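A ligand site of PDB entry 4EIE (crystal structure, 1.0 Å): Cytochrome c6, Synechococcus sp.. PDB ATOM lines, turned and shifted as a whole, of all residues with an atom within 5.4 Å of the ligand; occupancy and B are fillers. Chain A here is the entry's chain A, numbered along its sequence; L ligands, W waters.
SG of Cys 14 is covalently linked to C18 of the ligand, 1.8 Å away.
The side-chain sulfur (SG) of Cys 17 is bonded to a carbon (C25) of the ligand (1.9 Å).
FE1 of the ligand is bound by NE2 of His 18, at 2.0 Å.
An iron atom (FE1) of the ligand is bound by the side-chain sulfur of Met 58 (2.3 Å).
The backbone carbonyl oxygen (O) of Asn 30 lies close to an oxygen (O2) of the ligand (2.6 Å).
The guanidinium group (NH1) of Arg 26 is in salt-bridge range of an oxygen (O3) of the ligand (2.9 Å).
ND2 of Asn 39 lies within hydrogen-bond range of O1 of the ligand, at 3.5 Å.
The backbone NH (N) of Arg 26 sits at hydrogen-bond distance from the side-chain amide oxygen (OD1) of Asn 23 (3.0 Å).
The backbone carbonyl oxygen (O) of Met 36 sits at hydrogen-bond distance from the backbone NH (N) of Tyr 41, 2.8 Å away.
N of Tyr 61 is in hydrogen-bond range of O of Val 51.
The backbone carbonyl oxygen of Lys 29 lies within hydrogen-bond range of the side-chain amide nitrogen of Asn 23 (2.9 Å).
The side-chain amide oxygen (OD1) of Asn 39 sits at hydrogen-bond distance from the side-chain amino group (NZ) of Lys 29, 2.9 Å away.
OD1 of Asn 23 is in hydrogen-bond range of N of Val 25 (3.0 Å).
The side-chain amide nitrogen (ND2) of Asn 39 is in hydrogen-bond range of the backbone carbonyl oxygen (O) of Ala 35, 2.9 Å away.
Residues that only touch the ligand: Leu 50, Tyr 41, Tyr 61, Lys 29, Asn 23, Leu 31, Ala 35, His 13, Val 51, Lys 55, Met 36, Val 25 and Val 77.
Hydrophobic or aromatic side chains that line the ligand: His 18, Val 25, Leu 31, Ala 35, Met 36, Tyr 41, Leu 50, Val 51, Met 58, Tyr 61 and Val 77.
Within 4 Å of the ligand: His 13, Cys 14, Cys 17, His 18, Asn 23, Val 25, Arg 26, Lys 29, Asn 30, Leu 31, Ala 35, Met 36, Asn 39, Tyr 41, Leu 50, Val 51, Lys 55, Met 58, Tyr 61 and Val 77.
Water W1 lies within hydrogen-bond range of an oxygen (O3) of the ligand and the backbone NH of Asn 57.
Water W3 lies within hydrogen-bond range of NZ of Lys 29 (2.6 Å) and O4 of the ligand (2.7 Å).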
ATOM      1  N   PHE A  10      -2.844   8.860  10.818  1.00  0.00           N
ATOM      2  CA  PHE A  10      -1.931   7.739  10.835  1.00  0.00           C
ATOM      3  C   PHE A  10      -1.100   7.752  12.119  1.00  0.00           C
ATOM      4  O   PHE A  10      -0.953   6.733  12.783  1.00  0.00           O
ATOM      5  CB  PHE A  10      -1.007   7.758   9.593  1.00  0.00           C
ATOM      6  CG  PHE A  10      -0.186   6.514   9.469  1.00  0.00           C
ATOM      7  CD1 PHE A  10      -0.707   5.406   8.776  1.00  0.00           C
ATOM      8  CD2 PHE A  10       1.051   6.401  10.022  1.00  0.00           C
ATOM      9  CE1 PHE A  10       0.036   4.235   8.683  1.00  0.00           C
ATOM     10  CE2 PHE A  10       1.790   5.241   9.899  1.00  0.00           C
ATOM     11  CZ  PHE A  10       1.274   4.186   9.255  1.00  0.00           C
ATOM     12  N   HIS A  13      -3.419   6.739  15.124  1.00  0.00           N
ATOM     13  CA  HIS A  13      -4.194   5.521  15.159  1.00  0.00           C
ATOM     14  C   HIS A  13      -3.500   4.329  14.525  1.00  0.00           C
ATOM     15  O   HIS A  13      -3.969   3.214  14.718  1.00  0.00           O
ATOM     16  CB  HIS A  13      -5.512   5.689  14.431  1.00  0.00           C
ATOM     17  CG  HIS A  13      -6.380   6.666  15.108  1.00  0.00           C
ATOM     18  ND1 HIS A  13      -7.116   6.329  16.223  1.00  0.00           N
ATOM     19  CD2 HIS A  13      -6.545   7.984  14.902  1.00  0.00           C
ATOM     20  CE1 HIS A  13      -7.733   7.410  16.665  1.00  0.00           C
ATOM     21  NE2 HIS A  13      -7.414   8.412  15.872  1.00  0.00           N
ATOM     22  N   CYS A  14      -2.417   4.517  13.800  1.00  0.00           N
ATOM     23  CA  CYS A  14      -1.825   3.428  13.022  1.00  0.00           C
ATOM     24  C   CYS A  14      -0.361   3.187  13.337  1.00  0.00           C
ATOM     25  O   CYS A  14       0.124   2.077  13.167  1.00  0.00           O
ATOM     26  CB  CYS A  14      -1.957   3.695  11.505  1.00  0.00           C
ATOM     27  SG  CYS A  14      -3.560   4.300  10.966  1.00  0.00           S
ATOM     28  N   GLY A  16       1.305   2.920  15.983  1.00  0.00           N
ATOM     29  CA  GLY A  16       1.675   1.994  17.009  1.00  0.00           C
ATOM     30  C   GLY A  16       2.176   0.679  16.433  1.00  0.00           C
ATOM     31  O   GLY A  16       3.059   0.049  16.989  1.00  0.00           O
ATOM     32  N   CYS A  17       1.582   0.241  15.304  1.00  0.00           N
ATOM     33  CA  CYS A  17       1.985  -0.998  14.674  1.00  0.00           C
ATOM     34  C   CYS A  17       2.717  -0.810  13.361  1.00  0.00           C
ATOM     35  O   CYS A  17       3.423  -1.719  12.934  1.00  0.00           O
ATOM     36  CB  CYS A  17       0.754  -1.850  14.398  1.00  0.00           C
ATOM     37  SG  CYS A  17      -0.052  -2.221  15.981  1.00  0.00           S
ATOM     38  N   HIS A  18       2.512   0.335  12.716  1.00  0.00           N
ATOM     39  CA  HIS A  18       2.956   0.544  11.355  1.00  0.00           C
ATOM     40  C   HIS A  18       3.885   1.767  11.216  1.00  0.00           C
ATOM     41  O   HIS A  18       3.963   2.371  10.141  1.00  0.00           O
ATOM     42  CB  HIS A  18       1.801   0.737  10.379  1.00  0.00           C
ATOM     43  CG  HIS A  18       0.871  -0.439  10.272  1.00  0.00           C
ATOM     44  ND1 HIS A  18       1.223  -1.678   9.771  1.00  0.00           N
ATOM     45  CD2 HIS A  18      -0.463  -0.511  10.484  1.00  0.00           C
ATOM     46  CE1 HIS A  18       0.122  -2.428   9.673  1.00  0.00           C
ATOM     47  NE2 HIS A  18      -0.926  -1.771  10.079  1.00  0.00           N
ATOM     48  N   ASN A  23       5.314  -3.283  10.049  1.00  0.00           N
ATOM     49  CA  ASN A  23       4.246  -3.997  10.743  1.00  0.00           C
ATOM     50  C   ASN A  23       4.948  -4.809  11.815  1.00  0.00           C
ATOM     51  O   ASN A  23       5.481  -5.873  11.523  1.00  0.00           O
ATOM     52  CB  ASN A  23       3.413  -4.886   9.820  1.00  0.00           C
ATOM     53  CG  ASN A  23       2.217  -5.456  10.517  1.00  0.00           C
ATOM     54  OD1 ASN A  23       2.242  -5.601  11.744  1.00  0.00           O
ATOM     55  ND2 ASN A  23       1.157  -5.750   9.774  1.00  0.00           N
ATOM     56  N   VAL A  25       3.720  -6.406  14.200  1.00  0.00           N
ATOM     57  CA  VAL A  25       2.888  -7.526  14.625  1.00  0.00           C
ATOM     58  C   VAL A  25       3.042  -8.696  13.668  1.00  0.00           C
ATOM     59  O   VAL A  25       3.308  -9.814  14.093  1.00  0.00           O
ATOM     60  CB  VAL A  25       1.429  -7.079  14.731  1.00  0.00           C
ATOM     61  CG1 VAL A  25       0.543  -8.270  15.213  1.00  0.00           C
ATOM     62  CG2 VAL A  25       1.310  -5.896  15.688  1.00  0.00           C
ATOM     63  N   ARG A  26       2.796  -8.435  12.392  1.00  0.00           N
ATOM     64  CA  ARG A  26       2.801  -9.436  11.308  1.00  0.00           C
ATOM     65  C   ARG A  26       3.814  -8.944  10.323  1.00  0.00           C
ATOM     66  O   ARG A  26       3.551  -8.120   9.455  1.00  0.00           O
ATOM     67  CB  ARG A  26       1.432  -9.643  10.671  1.00  0.00           C
ATOM     68  CG  ARG A  26       1.415 -10.752   9.692  1.00  0.00           C
ATOM     69  CD  ARG A  26       0.059 -11.282   9.370  1.00  0.00           C
ATOM     70  NE  ARG A  26       0.166 -12.373   8.415  1.00  0.00           N
ATOM     71  CZ  ARG A  26      -0.843 -13.171   8.048  1.00  0.00           C
ATOM     72  NH1 ARG A  26      -2.077 -12.996   8.523  1.00  0.00           N
ATOM     73  NH2 ARG A  26      -0.603 -14.145   7.185  1.00  0.00           N
ATOM     74  N   GLY A  28       5.152 -10.049   7.655  1.00  0.00           N
ATOM     75  CA  GLY A  28       4.911 -10.137   6.238  1.00  0.00           C
ATOM     76  C   GLY A  28       3.789  -9.302   5.691  1.00  0.00           C
ATOM     77  O   GLY A  28       3.533  -9.416   4.474  1.00  0.00           O
ATOM     78  N   LYS A  29       3.213  -8.409   6.471  1.00  0.00           N
ATOM     79  CA  LYS A  29       2.111  -7.618   6.017  1.00  0.00           C
ATOM     80  C   LYS A  29       2.352  -6.155   6.347  1.00  0.00           C
ATOM     81  O   LYS A  29       1.524  -5.519   6.952  1.00  0.00           O
ATOM     82  CB  LYS A  29       0.797  -8.097   6.584  1.00  0.00           C
ATOM     83  CG  LYS A  29       0.428  -9.525   6.231  1.00  0.00           C
ATOM     84  CD  LYS A  29       0.038  -9.718   4.851  1.00  0.00           C
ATOM     85  CE  LYS A  29      -0.360 -11.153   4.503  1.00  0.00           C
ATOM     86  NZ  LYS A  29      -1.506 -11.090   3.621  1.00  0.00           N
ATOM     87  N   ASN A  30       3.465  -5.603   5.825  1.00  0.00           N
ATOM     88  CA  ASN A  30       3.722  -4.180   6.103  1.00  0.00           C
ATOM     89  C   ASN A  30       3.146  -3.270   5.011  1.00  0.00           C
ATOM     90  O   ASN A  30       2.386  -3.682   4.129  1.00  0.00           O
ATOM     91  CB  ASN A  30       5.213  -3.951   6.425  1.00  0.00           C
ATOM     92  CG  ASN A  30       6.131  -3.995   5.248  1.00  0.00           C
ATOM     93  OD1 ASN A  30       5.738  -3.795   4.100  1.00  0.00           O
ATOM     94  ND2 ASN A  30       7.421  -4.151   5.557  1.00  0.00           N
ATOM     95  N   LEU A  31       3.409  -1.972   5.169  1.00  0.00           N
ATOM     96  CA  LEU A  31       2.821  -0.959   4.317  1.00  0.00           C
ATOM     97  C   LEU A  31       3.786  -0.460   3.260  1.00  0.00           C
ATOM     98  O   LEU A  31       3.529   0.555   2.620  1.00  0.00           O
ATOM     99  CB  LEU A  31       2.276   0.226   5.140  1.00  0.00           C
ATOM    100  CG  LEU A  31       1.448  -0.119   6.363  1.00  0.00           C
ATOM    101  CD1 LEU A  31       0.838   1.167   6.910  1.00  0.00           C
ATOM    102  CD2 LEU A  31       0.425  -1.147   6.081  1.00  0.00           C
ATOM    103  N   ALA A  35       5.018  -5.625  -0.104  1.00  0.00           N
ATOM    104  CA  ALA A  35       3.911  -6.342   0.499  1.00  0.00           C
ATOM    105  C   ALA A  35       2.578  -5.751   0.083  1.00  0.00           C
ATOM    106  O   ALA A  35       1.597  -6.464  -0.137  1.00  0.00           O
ATOM    107  CB  ALA A  35       4.036  -6.309   2.015  1.00  0.00           C
ATOM    108  N   MET A  36       2.485  -4.405  -0.024  1.00  0.00           N
ATOM    109  CA  MET A  36       1.248  -3.786  -0.413  1.00  0.00           C
ATOM    110  C   MET A  36       0.861  -4.217  -1.846  1.00  0.00           C
ATOM    111  O   MET A  36      -0.300  -4.505  -2.107  1.00  0.00           O
ATOM    112  CB  MET A  36       1.379  -2.281  -0.308  1.00  0.00           C
ATOM    113  CG  MET A  36       1.484  -1.845   1.153  1.00  0.00           C
ATOM    114  SD  MET A  36      -0.077  -1.865   2.061  1.00  0.00           S
ATOM    115  CE  MET A  36      -0.783  -0.326   1.461  1.00  0.00           C
ATOM    116  N   ASN A  39      -0.289  -7.889  -2.004  1.00  0.00           N
ATOM    117  CA  ASN A  39      -1.604  -8.068  -1.426  1.00  0.00           C
ATOM    118  C   ASN A  39      -2.686  -7.211  -2.075  1.00  0.00           C
ATOM    119  O   ASN A  39      -3.819  -7.281  -1.687  1.00  0.00           O
ATOM    120  CB  ASN A  39      -1.506  -7.908   0.088  1.00  0.00           C
ATOM    121  CG  ASN A  39      -0.777  -9.012   0.745  1.00  0.00           C
ATOM    122  OD1 ASN A  39      -1.345 -10.108   0.918  1.00  0.00           O
ATOM    123  ND2 ASN A  39       0.429  -8.753   1.172  1.00  0.00           N
ATOM    124  N   TYR A  41      -3.075  -3.888  -2.145  1.00  0.00           N
ATOM    125  CA  TYR A  41      -3.431  -2.624  -1.506  1.00  0.00           C
ATOM    126  C   TYR A  41      -2.772  -1.496  -2.281  1.00  0.00           C
ATOM    127  O   TYR A  41      -1.828  -0.826  -1.850  1.00  0.00           O
ATOM    128  CB  TYR A  41      -2.963  -2.640  -0.043  1.00  0.00           C
ATOM    129  CG  TYR A  41      -3.748  -3.622   0.772  1.00  0.00           C
ATOM    130  CD1 TYR A  41      -5.078  -3.374   1.069  1.00  0.00           C
ATOM    131  CD2 TYR A  41      -3.224  -4.826   1.221  1.00  0.00           C
ATOM    132  CE1 TYR A  41      -5.829  -4.258   1.796  1.00  0.00           C
ATOM    133  CE2 TYR A  41      -3.983  -5.735   1.906  1.00  0.00           C
ATOM    134  CZ  TYR A  41      -5.296  -5.457   2.164  1.00  0.00           C
ATOM    135  OH  TYR A  41      -6.061  -6.372   2.845  1.00  0.00           O
ATOM    136  N   ILE A  47      -7.496  -0.111   0.516  1.00  0.00           N
ATOM    137  CA  ILE A  47      -7.011   0.211   1.835  1.00  0.00           C
ATOM    138  C   ILE A  47      -8.127   0.611   2.789  1.00  0.00           C
ATOM    139  O   ILE A  47      -8.196   0.136   3.915  1.00  0.00           O
ATOM    140  CB  ILE A  47      -5.912   1.299   1.750  1.00  0.00           C
ATOM    141  CG1 ILE A  47      -4.700   0.780   0.991  1.00  0.00           C
ATOM    142  CG2 ILE A  47      -5.487   1.787   3.142  1.00  0.00           C
ATOM    143  CD1 ILE A  47      -3.787   1.861   0.449  1.00  0.00           C
ATOM    144  N   LEU A  50     -10.098  -2.353   4.161  1.00  0.00           N
ATOM    145  CA  LEU A  50      -9.383  -3.032   5.253  1.00  0.00           C
ATOM    146  C   LEU A  50      -9.465  -2.204   6.517  1.00  0.00           C
ATOM    147  O   LEU A  50      -9.725  -2.723   7.596  1.00  0.00           O
ATOM    148  CB  LEU A  50      -7.972  -3.290   4.883  1.00  0.00           C
ATOM    149  CG  LEU A  50      -7.093  -3.874   5.994  1.00  0.00           C
ATOM    150  CD1 LEU A  50      -7.630  -5.156   6.576  1.00  0.00           C
ATOM    151  CD2 LEU A  50      -5.686  -4.018   5.543  1.00  0.00           C
ATOM    152  N   VAL A  51      -9.188  -0.898   6.437  1.00  0.00           N
ATOM    153  CA  VAL A  51      -9.227  -0.087   7.644  1.00  0.00           C
ATOM    154  C   VAL A  51     -10.596  -0.128   8.263  1.00  0.00           C
ATOM    155  O   VAL A  51     -10.744  -0.183   9.476  1.00  0.00           O
ATOM    156  CB  VAL A  51      -8.810   1.357   7.283  1.00  0.00           C
ATOM    157  CG1 VAL A  51      -9.046   2.285   8.432  1.00  0.00           C
ATOM    158  CG2 VAL A  51      -7.298   1.386   6.913  1.00  0.00           C
ATOM    159  N   LYS A  55      -8.995  -6.892   9.995  1.00  0.00           N
ATOM    160  CA  LYS A  55      -8.656  -8.240   9.528  1.00  0.00           C
ATOM    161  C   LYS A  55      -7.717  -8.848  10.506  1.00  0.00           C
ATOM    162  O   LYS A  55      -6.708  -8.269  10.904  1.00  0.00           O
ATOM    163  CB  LYS A  55      -7.953  -8.158   8.200  1.00  0.00           C
ATOM    164  CG  LYS A  55      -7.637  -9.521   7.636  1.00  0.00           C
ATOM    165  CD  LYS A  55      -7.191  -9.411   6.231  1.00  0.00           C
ATOM    166  CE  LYS A  55      -7.039 -10.820   5.693  1.00  0.00           C
ATOM    167  NZ  LYS A  55      -6.778 -10.766   4.248  1.00  0.00           N
ATOM    168  N   GLY A  56      -8.046 -10.054  10.988  1.00  0.00           N
ATOM    169  CA  GLY A  56      -7.155 -10.817  11.831  1.00  0.00           C
ATOM    170  C   GLY A  56      -6.914  -9.998  13.080  1.00  0.00           C
ATOM    171  O   GLY A  56      -7.851  -9.545  13.770  1.00  0.00           O
ATOM    172  N   ASN A  57      -5.622  -9.818  13.412  1.00  0.00           N
ATOM    173  CA  ASN A  57      -5.269  -9.100  14.602  1.00  0.00           C
ATOM    174  C   ASN A  57      -5.317  -7.585  14.468  1.00  0.00           C
ATOM    175  O   ASN A  57      -5.051  -6.904  15.442  1.00  0.00           O
ATOM    176  CB  ASN A  57      -3.918  -9.596  15.121  1.00  0.00           C
ATOM    177  CG  ASN A  57      -3.987 -11.021  15.610  1.00  0.00           C
ATOM    178  OD1 ASN A  57      -4.949 -11.396  16.291  1.00  0.00           O
ATOM    179  ND2 ASN A  57      -3.000 -11.813  15.227  1.00  0.00           N
ATOM    180  N   MET A  58      -5.611  -7.070  13.264  1.00  0.00           N
ATOM    181  CA  MET A  58      -5.859  -5.639  13.104  1.00  0.00           C
ATOM    182  C   MET A  58      -7.315  -5.345  13.361  1.00  0.00           C
ATOM    183  O   MET A  58      -8.213  -5.947  12.762  1.00  0.00           O
ATOM    184  CB  MET A  58      -5.472  -5.179  11.703  1.00  0.00           C
ATOM    185  CG  MET A  58      -5.663  -3.677  11.523  1.00  0.00           C
ATOM    186  SD  MET A  58      -5.027  -3.152   9.921  1.00  0.00           S
ATOM    187  CE  MET A  58      -6.135  -1.764   9.584  1.00  0.00           C
ATOM    188  N   TYR A  61     -11.766  -0.215  12.146  1.00  0.00           N
ATOM    189  CA  TYR A  61     -11.837   1.200  12.488  1.00  0.00           C
ATOM    190  C   TYR A  61     -13.137   1.826  12.026  1.00  0.00           C
ATOM    191  O   TYR A  61     -13.336   3.025  12.270  1.00  0.00           O
ATOM    192  CB  TYR A  61     -10.626   1.992  11.945  1.00  0.00           C
ATOM    193  CG  TYR A  61      -9.355   1.578  12.634  1.00  0.00           C
ATOM    194  CD1 TYR A  61      -8.666   0.433  12.263  1.00  0.00           C
ATOM    195  CD2 TYR A  61      -8.877   2.294  13.724  1.00  0.00           C
ATOM    196  CE1 TYR A  61      -7.551   0.000  12.950  1.00  0.00           C
ATOM    197  CE2 TYR A  61      -7.773   1.861  14.447  1.00  0.00           C
ATOM    198  CZ  TYR A  61      -7.127   0.731  14.070  1.00  0.00           C
ATOM    199  OH  TYR A  61      -6.037   0.228  14.756  1.00  0.00           O
ATOM    200  N   LEU A  65     -13.174   5.711  13.453  1.00  0.00           N
ATOM    201  CA  LEU A  65     -12.814   6.806  12.569  1.00  0.00           C
ATOM    202  C   LEU A  65     -13.987   7.033  11.615  1.00  0.00           C
ATOM    203  O   LEU A  65     -14.622   6.095  11.209  1.00  0.00           O
ATOM    204  CB  LEU A  65     -11.554   6.451  11.767  1.00  0.00           C
ATOM    205  CG  LEU A  65     -10.293   6.299  12.611  1.00  0.00           C
ATOM    206  CD1 LEU A  65      -9.182   5.767  11.688  1.00  0.00           C
ATOM    207  CD2 LEU A  65      -9.882   7.604  13.259  1.00  0.00           C
ATOM    208  N   VAL A  73      -6.694   8.785   5.696  1.00  0.00           N
ATOM    209  CA  VAL A  73      -5.557   7.960   6.105  1.00  0.00           C
ATOM    210  C   VAL A  73      -5.233   6.938   4.985  1.00  0.00           C
ATOM    211  O   VAL A  73      -4.082   6.574   4.800  1.00  0.00           O
ATOM    212  CB  VAL A  73      -5.760   7.328   7.465  1.00  0.00           C
ATOM    213  CG1 VAL A  73      -6.761   6.151   7.472  1.00  0.00           C
ATOM    214  CG2 VAL A  73      -4.416   6.868   8.032  1.00  0.00           C
ATOM    215  N   VAL A  77      -1.617   6.389   3.259  1.00  0.00           N
ATOM    216  CA  VAL A  77      -0.954   5.127   3.158  1.00  0.00           C
ATOM    217  C   VAL A  77      -0.659   4.726   1.732  1.00  0.00           C
ATOM    218  O   VAL A  77       0.421   4.207   1.422  1.00  0.00           O
ATOM    219  CB  VAL A  77      -1.760   4.032   3.895  1.00  0.00           C
ATOM    220  CG1 VAL A  77      -1.253   2.626   3.597  1.00  0.00           C
ATOM    221  CG2 VAL A  77      -1.720   4.292   5.375  1.00  0.00           C
HETATM  222 FE1  LIG L   1      -2.822  -2.364  10.068  1.00  0.00          FE
HETATM  223  C1  LIG L   1      -2.368  -4.929   7.917  1.00  0.00           C
HETATM  224  C2  LIG L   1      -3.329  -0.242   7.443  1.00  0.00           C
HETATM  225  C3  LIG L   1      -3.658   0.132  12.225  1.00  0.00           C
HETATM  226  C4  LIG L   1      -1.937  -4.343  12.642  1.00  0.00           C
HETATM  227  N1  LIG L   1      -2.786  -2.550   8.098  1.00  0.00           N
HETATM  228  C5  LIG L   1      -2.532  -3.688   7.366  1.00  0.00           C
HETATM  229  C6  LIG L   1      -2.535  -3.413   5.963  1.00  0.00           C
HETATM  230  C7  LIG L   1      -2.823  -2.088   5.824  1.00  0.00           C
HETATM  231  C8  LIG L   1      -3.004  -1.564   7.151  1.00  0.00           C
HETATM  232  C9  LIG L   1      -2.994  -1.291   4.556  1.00  0.00           C
HETATM  233  C10 LIG L   1      -2.237  -4.413   4.868  1.00  0.00           C
HETATM  234  C11 LIG L   1      -0.731  -4.564   4.676  1.00  0.00           C
HETATM  235  C12 LIG L   1      -0.319  -5.648   3.728  1.00  0.00           C
HETATM  236  O1  LIG L   1      -1.118  -6.507   3.351  1.00  0.00           O
HETATM  237  O2  LIG L   1       0.906  -5.730   3.354  1.00  0.00           O
HETATM  238  N2  LIG L   1      -3.416  -0.464   9.883  1.00  0.00           N
HETATM  239  C13 LIG L   1      -3.547   0.239   8.725  1.00  0.00           C
HETATM  240  C14 LIG L   1      -3.998   1.595   8.993  1.00  0.00           C
HETATM  241  C15 LIG L   1      -4.181   1.663  10.323  1.00  0.00           C
HETATM  242  C16 LIG L   1      -3.773   0.381  10.879  1.00  0.00           C
HETATM  243  C17 LIG L   1      -4.162   2.664   7.973  1.00  0.00           C
HETATM  244  C18 LIG L   1      -4.661   2.835  11.204  1.00  0.00           C
HETATM  245  C19 LIG L   1      -6.051   3.252  10.920  1.00  0.00           C
HETATM  246  N3  LIG L   1      -2.801  -2.175  12.046  1.00  0.00           N
HETATM  247  C20 LIG L   1      -3.087  -1.045  12.745  1.00  0.00           C
HETATM  248  C21 LIG L   1      -2.709  -1.194  14.121  1.00  0.00           C
HETATM  249  C22 LIG L   1      -2.210  -2.435  14.251  1.00  0.00           C
HETATM  250  C23 LIG L   1      -2.289  -3.069  12.948  1.00  0.00           C
HETATM  251  C24 LIG L   1      -2.753  -0.064  15.133  1.00  0.00           C
HETATM  252  C25 LIG L   1      -1.596  -3.110  15.470  1.00  0.00           C
HETATM  253  C26 LIG L   1      -2.479  -3.169  16.628  1.00  0.00           C
HETATM  254  N4  LIG L   1      -2.285  -4.255  10.255  1.00  0.00           N
HETATM  255  C27 LIG L   1      -2.032  -4.964  11.407  1.00  0.00           C
HETATM  256  C28 LIG L   1      -1.907  -6.339  11.195  1.00  0.00           C
HETATM  257  C29 LIG L   1      -2.107  -6.529   9.833  1.00  0.00           C
HETATM  258  C30 LIG L   1      -2.279  -5.236   9.269  1.00  0.00           C
HETATM  259  C31 LIG L   1      -1.681  -7.399  12.226  1.00  0.00           C
HETATM  260  C32 LIG L   1      -2.158  -7.842   9.101  1.00  0.00           C
HETATM  261  C33 LIG L   1      -3.612  -8.269   8.902  1.00  0.00           C
HETATM  262  C34 LIG L   1      -3.625  -9.653   8.294  1.00  0.00           C
HETATM  263  O3  LIG L   1      -3.705 -10.652   9.000  1.00  0.00           O
HETATM  264  O4  LIG L   1      -3.442  -9.781   7.105  1.00  0.00           O
HETATM  265  O   HOH W   1      -3.478 -10.885  11.630  1.00  0.00           O
HETATM  266  O   HOH W   2      -5.594 -12.706   8.793  1.00  0.00           O
HETATM  267  O   HOH W   3      -3.457 -11.707   5.228  1.00  0.00           O
HETATM  268  O   HOH W   4      -3.206  -7.754   5.220  1.00  0.00           O
